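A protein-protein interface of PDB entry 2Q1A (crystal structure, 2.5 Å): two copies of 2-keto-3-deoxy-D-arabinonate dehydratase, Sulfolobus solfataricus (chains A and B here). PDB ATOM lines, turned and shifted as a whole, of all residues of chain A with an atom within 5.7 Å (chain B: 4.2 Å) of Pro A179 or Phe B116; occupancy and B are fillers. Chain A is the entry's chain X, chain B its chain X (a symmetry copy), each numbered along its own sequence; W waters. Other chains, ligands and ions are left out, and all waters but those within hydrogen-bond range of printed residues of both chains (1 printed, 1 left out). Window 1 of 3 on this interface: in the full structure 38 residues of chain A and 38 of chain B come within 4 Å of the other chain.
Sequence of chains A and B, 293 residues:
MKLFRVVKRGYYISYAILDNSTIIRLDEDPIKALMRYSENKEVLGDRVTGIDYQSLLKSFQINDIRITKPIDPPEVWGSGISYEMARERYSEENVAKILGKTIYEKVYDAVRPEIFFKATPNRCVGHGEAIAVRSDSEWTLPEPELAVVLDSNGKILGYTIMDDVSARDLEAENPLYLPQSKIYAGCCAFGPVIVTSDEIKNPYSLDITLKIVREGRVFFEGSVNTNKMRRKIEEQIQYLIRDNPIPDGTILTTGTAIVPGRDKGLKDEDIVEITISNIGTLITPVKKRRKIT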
ATOM      1  N   PRO A 175      17.748  19.616  13.668  1.00  0.00           N
ATOM      2  CA  PRO A 175      16.697  20.105  14.583  1.00  0.00           C
ATOM      3  C   PRO A 175      15.527  19.129  14.781  1.00  0.00           C
ATOM      4  O   PRO A 175      14.730  19.310  15.702  1.00  0.00           O
ATOM      5  CB  PRO A 175      16.218  21.402  13.921  1.00  0.00           C
ATOM      6  CG  PRO A 175      16.649  21.295  12.479  1.00  0.00           C
ATOM      7  CD  PRO A 175      17.928  20.505  12.503  1.00  0.00           C
ATOM      8  N   LEU A 176      15.440  18.103  13.935  1.00  0.00           N
ATOM      9  CA  LEU A 176      14.424  17.058  14.082  1.00  0.00           C
ATOM     10  C   LEU A 176      14.752  16.092  15.215  1.00  0.00           C
ATOM     11  O   LEU A 176      13.908  15.292  15.626  1.00  0.00           O
ATOM     12  CB  LEU A 176      14.223  16.290  12.769  1.00  0.00           C
ATOM     13  CG  LEU A 176      13.576  17.054  11.601  1.00  0.00           C
ATOM     14  CD1 LEU A 176      13.317  16.144  10.391  1.00  0.00           C
ATOM     15  CD2 LEU A 176      12.283  17.742  12.036  1.00  0.00           C
ATOM     16  N   TYR A 177      15.978  16.173  15.719  1.00  0.00           N
ATOM     17  CA  TYR A 177      16.417  15.341  16.836  1.00  0.00           C
ATOM     18  C   TYR A 177      16.154  16.007  18.193  1.00  0.00           C
ATOM     19  O   TYR A 177      16.439  15.429  19.239  1.00  0.00           O
ATOM     20  CB  TYR A 177      17.902  14.991  16.684  1.00  0.00           C
ATOM     21  CG  TYR A 177      18.229  14.111  15.489  1.00  0.00           C
ATOM     22  CD1 TYR A 177      17.332  13.137  15.043  1.00  0.00           C
ATOM     23  CD2 TYR A 177      19.454  14.228  14.829  1.00  0.00           C
ATOM     24  CE1 TYR A 177      17.629  12.321  13.961  1.00  0.00           C
ATOM     25  CE2 TYR A 177      19.767  13.414  13.735  1.00  0.00           C
ATOM     26  CZ  TYR A 177      18.847  12.461  13.307  1.00  0.00           C
ATOM     27  OH  TYR A 177      19.137  11.645  12.229  1.00  0.00           O
ATOM     28  N   LEU A 178      15.589  17.210  18.165  1.00  0.00           N
ATOM     29  CA  LEU A 178      15.343  17.998  19.373  1.00  0.00           C
ATOM     30  C   LEU A 178      14.619  17.245  20.513  1.00  0.00           C
ATOM     31  O   LEU A 178      15.068  17.308  21.660  1.00  0.00           O
ATOM     32  CB  LEU A 178      14.641  19.310  19.012  1.00  0.00           C
ATOM     33  CG  LEU A 178      14.745  20.568  19.884  1.00  0.00           C
ATOM     34  CD1 LEU A 178      16.156  20.860  20.382  1.00  0.00           C
ATOM     35  CD2 LEU A 178      14.216  21.767  19.105  1.00  0.00           C
ATOM     36  N   PRO A 179      13.523  16.507  20.207  1.00  0.00           N
ATOM     37  CA  PRO A 179      12.859  15.748  21.279  1.00  0.00           C
ATOM     38  C   PRO A 179      13.745  14.680  21.936  1.00  0.00           C
ATOM     39  O   PRO A 179      13.647  14.465  23.146  1.00  0.00           O
ATOM     40  CB  PRO A 179      11.673  15.084  20.568  1.00  0.00           C
ATOM     41  CG  PRO A 179      11.473  15.870  19.326  1.00  0.00           C
ATOM     42  CD  PRO A 179      12.829  16.326  18.916  1.00  0.00           C
ATOM     43  N   GLN A 180      14.584  14.010  21.152  1.00  0.00           N
ATOM     44  CA  GLN A 180      15.546  13.044  21.704  1.00  0.00           C
ATOM     45  C   GLN A 180      16.604  13.738  22.565  1.00  0.00           C
ATOM     46  O   GLN A 180      17.087  13.173  23.546  1.00  0.00           O
ATOM     47  CB  GLN A 180      16.245  12.259  20.594  1.00  0.00           C
ATOM     48  CG  GLN A 180      15.326  11.424  19.732  1.00  0.00           C
ATOM     49  CD  GLN A 180      16.099  10.573  18.740  1.00  0.00           C
ATOM     50  OE1 GLN A 180      16.927   9.744  19.125  1.00  0.00           O
ATOM     51  NE2 GLN A 180      15.828  10.774  17.452  1.00  0.00           N
ATOM     52  N   SER A 181      16.943  14.968  22.183  1.00  0.00           N
ATOM     53  CA  SER A 181      17.952  15.753  22.877  1.00  0.00           C
ATOM     54  C   SER A 181      17.435  16.311  24.198  1.00  0.00           C
ATOM     55  O   SER A 181      18.236  16.688  25.059  1.00  0.00           O
ATOM     56  CB  SER A 181      18.437  16.906  21.984  1.00  0.00           C
ATOM     57  OG  SER A 181      17.621  18.058  22.130  1.00  0.00           O
ATOM     58  N   LYS A 182      16.107  16.358  24.347  1.00  0.00           N
ATOM     59  CA  LYS A 182      15.456  17.062  25.461  1.00  0.00           C
ATOM     60  C   LYS A 182      14.706  16.181  26.471  1.00  0.00           C
ATOM     61  O   LYS A 182      14.544  16.573  27.629  1.00  0.00           O
ATOM     62  CB  LYS A 182      14.504  18.137  24.918  1.00  0.00           C
ATOM     63  CG  LYS A 182      15.181  19.339  24.260  1.00  0.00           C
ATOM     64  CD  LYS A 182      15.440  20.456  25.244  1.00  0.00           C
ATOM     65  CE  LYS A 182      16.200  21.597  24.591  1.00  0.00           C
ATOM     66  NZ  LYS A 182      16.443  22.741  25.533  1.00  0.00           N
ATOM     67  N   ILE A 183      14.260  15.000  26.036  1.00  0.00           N
ATOM     68  CA  ILE A 183      13.306  14.176  26.799  1.00  0.00           C
ATOM     69  C   ILE A 183      13.866  12.788  27.062  1.00  0.00           C
ATOM     70  O   ILE A 183      13.986  11.973  26.142  1.00  0.00           O
ATOM     71  CB  ILE A 183      11.927  14.008  26.049  1.00  0.00           C
ATOM     72  CG1 ILE A 183      11.390  15.349  25.534  1.00  0.00           C
ATOM     73  CG2 ILE A 183      10.892  13.327  26.945  1.00  0.00           C
ATOM     74  CD1 ILE A 183      10.313  15.211  24.452  1.00  0.00           C
ATOM     75  N   TYR A 184      14.183  12.523  28.327  1.00  0.00           N
ATOM     76  CA  TYR A 184      14.776  11.254  28.754  1.00  0.00           C
ATOM     77  C   TYR A 184      14.889  11.227  30.279  1.00  0.00           C
ATOM     78  O   TYR A 184      14.665  12.248  30.943  1.00  0.00           O
ATOM     79  CB  TYR A 184      16.156  11.041  28.098  1.00  0.00           C
ATOM     80  CG  TYR A 184      17.182  12.128  28.374  1.00  0.00           C
ATOM     81  CD1 TYR A 184      18.106  11.988  29.413  1.00  0.00           C
ATOM     82  CD2 TYR A 184      17.251  13.280  27.584  1.00  0.00           C
ATOM     83  CE1 TYR A 184      19.067  12.974  29.674  1.00  0.00           C
ATOM     84  CE2 TYR A 184      18.211  14.276  27.833  1.00  0.00           C
ATOM     85  CZ  TYR A 184      19.115  14.112  28.889  1.00  0.00           C
ATOM     86  OH  TYR A 184      20.067  15.077  29.164  1.00  0.00           O
ATOM     87  N   TRP B  77       4.059   8.259  21.242  1.00  0.00           N
ATOM     88  CA  TRP B  77       5.195   8.815  20.509  1.00  0.00           C
ATOM     89  C   TRP B  77       5.071   8.547  19.017  1.00  0.00           C
ATOM     90  O   TRP B  77       4.496   7.536  18.591  1.00  0.00           O
ATOM     91  CB  TRP B  77       6.523   8.237  21.003  1.00  0.00           C
ATOM     92  CG  TRP B  77       6.892   8.558  22.422  1.00  0.00           C
ATOM     93  CD1 TRP B  77       6.321   8.053  23.550  1.00  0.00           C
ATOM     94  CD2 TRP B  77       7.957   9.413  22.862  1.00  0.00           C
ATOM     95  NE1 TRP B  77       6.947   8.548  24.667  1.00  0.00           N
ATOM     96  CE2 TRP B  77       7.960   9.382  24.275  1.00  0.00           C
ATOM     97  CE3 TRP B  77       8.911  10.201  22.201  1.00  0.00           C
ATOM     98  CZ2 TRP B  77       8.869  10.117  25.041  1.00  0.00           C
ATOM     99  CZ3 TRP B  77       9.816  10.933  22.967  1.00  0.00           C
ATOM    100  CH2 TRP B  77       9.788  10.880  24.371  1.00  0.00           C
ATOM    101  N   GLY B  78       5.635   9.461  18.232  1.00  0.00           N
ATOM    102  CA  GLY B  78       5.640   9.341  16.785  1.00  0.00           C
ATOM    103  C   GLY B  78       7.018   9.149  16.185  1.00  0.00           C
ATOM    104  O   GLY B  78       8.037   9.521  16.777  1.00  0.00           O
ATOM    105  N   SER B  79       7.040   8.555  15.000  1.00  0.00           N
ATOM    106  CA  SER B  79       8.253   8.420  14.222  1.00  0.00           C
ATOM    107  C   SER B  79       8.044   9.178  12.922  1.00  0.00           C
ATOM    108  O   SER B  79       6.927   9.250  12.416  1.00  0.00           O
ATOM    109  CB  SER B  79       8.523   6.954  13.939  1.00  0.00           C
ATOM    110  OG  SER B  79       9.912   6.718  13.835  1.00  0.00           O
ATOM    111  N   GLU B 114      13.912   9.946  13.143  1.00  0.00           N
ATOM    112  CA  GLU B 114      13.177  10.967  13.863  1.00  0.00           C
ATOM    113  C   GLU B 114      12.192  10.310  14.827  1.00  0.00           C
ATOM    114  O   GLU B 114      11.477   9.374  14.456  1.00  0.00           O
ATOM    115  CB  GLU B 114      12.445  11.897  12.900  1.00  0.00           C
ATOM    116  CG  GLU B 114      11.865  13.145  13.569  1.00  0.00           C
ATOM    117  CD  GLU B 114      10.800  13.828  12.731  1.00  0.00           C
ATOM    118  OE1 GLU B 114      10.634  13.451  11.546  1.00  0.00           O
ATOM    119  OE2 GLU B 114      10.133  14.746  13.260  1.00  0.00           O
ATOM    120  N   ILE B 115      12.199  10.793  16.067  1.00  0.00           N
ATOM    121  CA  ILE B 115      11.272  10.370  17.109  1.00  0.00           C
ATOM    122  C   ILE B 115      10.839  11.632  17.852  1.00  0.00           C
ATOM    123  O   ILE B 115      11.684  12.444  18.248  1.00  0.00           O
ATOM    124  CB  ILE B 115      11.950   9.391  18.118  1.00  0.00           C
ATOM    125  CG1 ILE B 115      12.577   8.179  17.408  1.00  0.00           C
ATOM    126  CG2 ILE B 115      10.988   8.974  19.244  1.00  0.00           C
ATOM    127  CD1 ILE B 115      11.610   7.090  16.976  1.00  0.00           C
ATOM    128  N   PHE B 116       9.526  11.801  18.022  1.00  0.00           N
ATOM    129  CA  PHE B 116       8.977  12.960  18.734  1.00  0.00           C
ATOM    130  C   PHE B 116       7.871  12.539  19.694  1.00  0.00           C
ATOM    131  O   PHE B 116       7.305  11.450  19.556  1.00  0.00           O
ATOM    132  CB  PHE B 116       8.469  14.022  17.747  1.00  0.00           C
ATOM    133  CG  PHE B 116       7.387  13.528  16.818  1.00  0.00           C
ATOM    134  CD1 PHE B 116       6.041  13.725  17.127  1.00  0.00           C
ATOM    135  CD2 PHE B 116       7.715  12.861  15.636  1.00  0.00           C
ATOM    136  CE1 PHE B 116       5.032  13.258  16.279  1.00  0.00           C
ATOM    137  CE2 PHE B 116       6.714  12.386  14.779  1.00  0.00           C
ATOM    138  CZ  PHE B 116       5.366  12.588  15.101  1.00  0.00           C
ATOM    139  N   PHE B 117       7.577  13.397  20.672  1.00  0.00           N
ATOM    140  CA  PHE B 117       6.463  13.155  21.591  1.00  0.00           C
ATOM    141  C   PHE B 117       5.162  13.608  20.946  1.00  0.00           C
ATOM    142  O   PHE B 117       5.058  14.745  20.464  1.00  0.00           O
ATOM    143  CB  PHE B 117       6.675  13.872  22.930  1.00  0.00           C
ATOM    144  CG  PHE B 117       5.632  13.540  23.967  1.00  0.00           C
ATOM    145  CD1 PHE B 117       4.606  14.440  24.260  1.00  0.00           C
ATOM    146  CD2 PHE B 117       5.663  12.322  24.642  1.00  0.00           C
ATOM    147  CE1 PHE B 117       3.632  14.137  25.217  1.00  0.00           C
ATOM    148  CE2 PHE B 117       4.684  12.008  25.598  1.00  0.00           C
ATOM    149  CZ  PHE B 117       3.669  12.918  25.882  1.00  0.00           C
ATOM    150  N   LYS B 118       4.171  12.724  20.945  1.00  0.00           N
ATOM    151  CA  LYS B 118       2.919  12.978  20.228  1.00  0.00           C
ATOM    152  C   LYS B 118       1.754  13.426  21.111  1.00  0.00           C
ATOM    153  O   LYS B 118       1.146  14.466  20.835  1.00  0.00           O
ATOM    154  CB  LYS B 118       2.522  11.770  19.368  1.00  0.00           C
ATOM    155  CG  LYS B 118       1.182  11.914  18.648  1.00  0.00           C
ATOM    156  CD  LYS B 118       1.147  13.122  17.715  1.00  0.00           C
ATOM    157  CE  LYS B 118      -0.281  13.455  17.316  1.00  0.00           C
ATOM    158  NZ  LYS B 118      -0.354  14.625  16.391  1.00  0.00           N
ATOM    159  N   ASP B 164      -2.070  10.558  13.060  1.00  0.00           N
ATOM    160  CA  ASP B 164      -1.177  11.612  13.533  1.00  0.00           C
ATOM    161  C   ASP B 164      -1.604  12.970  12.944  1.00  0.00           C
ATOM    162  O   ASP B 164      -1.025  13.473  11.976  1.00  0.00           O
ATOM    163  CB  ASP B 164       0.295  11.249  13.220  1.00  0.00           C
ATOM    164  CG  ASP B 164       1.280  12.384  13.516  1.00  0.00           C
ATOM    165  OD1 ASP B 164       1.001  13.260  14.358  1.00  0.00           O
ATOM    166  OD2 ASP B 164       2.359  12.394  12.892  1.00  0.00           O
ATOM    167  N   LYS B 182       1.759  19.443  16.516  1.00  0.00           N
ATOM    168  CA  LYS B 182       1.514  18.015  16.759  1.00  0.00           C
ATOM    169  C   LYS B 182       0.746  17.670  18.044  1.00  0.00           C
ATOM    170  O   LYS B 182       0.099  16.623  18.112  1.00  0.00           O
ATOM    171  CB  LYS B 182       2.840  17.243  16.735  1.00  0.00           C
ATOM    172  CG  LYS B 182       3.504  17.125  15.363  1.00  0.00           C
ATOM    173  CD  LYS B 182       3.079  15.874  14.631  1.00  0.00           C
ATOM    174  CE  LYS B 182       3.673  15.828  13.233  1.00  0.00           C
ATOM    175  NZ  LYS B 182       3.299  14.578  12.489  1.00  0.00           N
HETATM  176  O   HOH W   1      11.026  16.240  15.612  1.00  0.00           O
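The side-chain hydroxyl of Ser B79 is in hydrogen-bond range of the backbone carbonyl oxygen of Glu B114, 3.1 Å away. N of Gly B78 lies within hydrogen-bond range of O of Phe B116, 2.9 Å away.
O of Leu A176 touches CG of Glu B114, 3.6 Å away. O of Ile B115 touches CB of Pro A179, at 3.5 Å. Pro A179 touches Phe B116. Gln A180 touches Ile B115 (NE2 to N, 3.9 Å). Ile A183 touches Trp B77 (CG2 to CH2, 3.7 Å).
Phe B116 touches one residue of chain A. Printed residues of chain A within 4 Å of Trp B77: Ile A183. Of the printed residues of chain A, Glu B114 touches Leu A176. Printed residues of chain B within 4 Å of Ile A183: Trp B77. Of the printed residues of chain B, Leu A176 touches Glu B114 (3.6 Å). Tyr A184 touches none of the printed residues of chain B. The nearest printed residue of chain A that does not touch Phe B116 is Leu A176 (6.0 Å). The nearest printed residue of chain B that does not touch Gln A180 is Glu B114 (4.5 Å).
Printed residues of chain B that touch a printed residue of chain A: Trp B77, Glu B114, Ile B115 and Phe B116. Hydrophobic or aromatic side chains of chain B that line the printed part of chain A: Trp B77 and Phe B116. Of the 10 printed residues of chain A, 4 touch a printed residue of chain B. Printed residues of chain A that touch a printed residue of chain B: Leu A176, Pro A179, Gln A180 and Ile A183. Among the printed residues, 5 pairs touch across the chains. Among the printed residues, no Asp or Glu carboxylate lies within 4 Å of a Lys or Arg side-chain nitrogen of the other chain.
Position printed for both chains: 182.
Water W1 lies within hydrogen-bond range of the side-chain carboxylate (OE2) of Glu B114 and the backbone carbonyl oxygen (O) of Leu A176.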
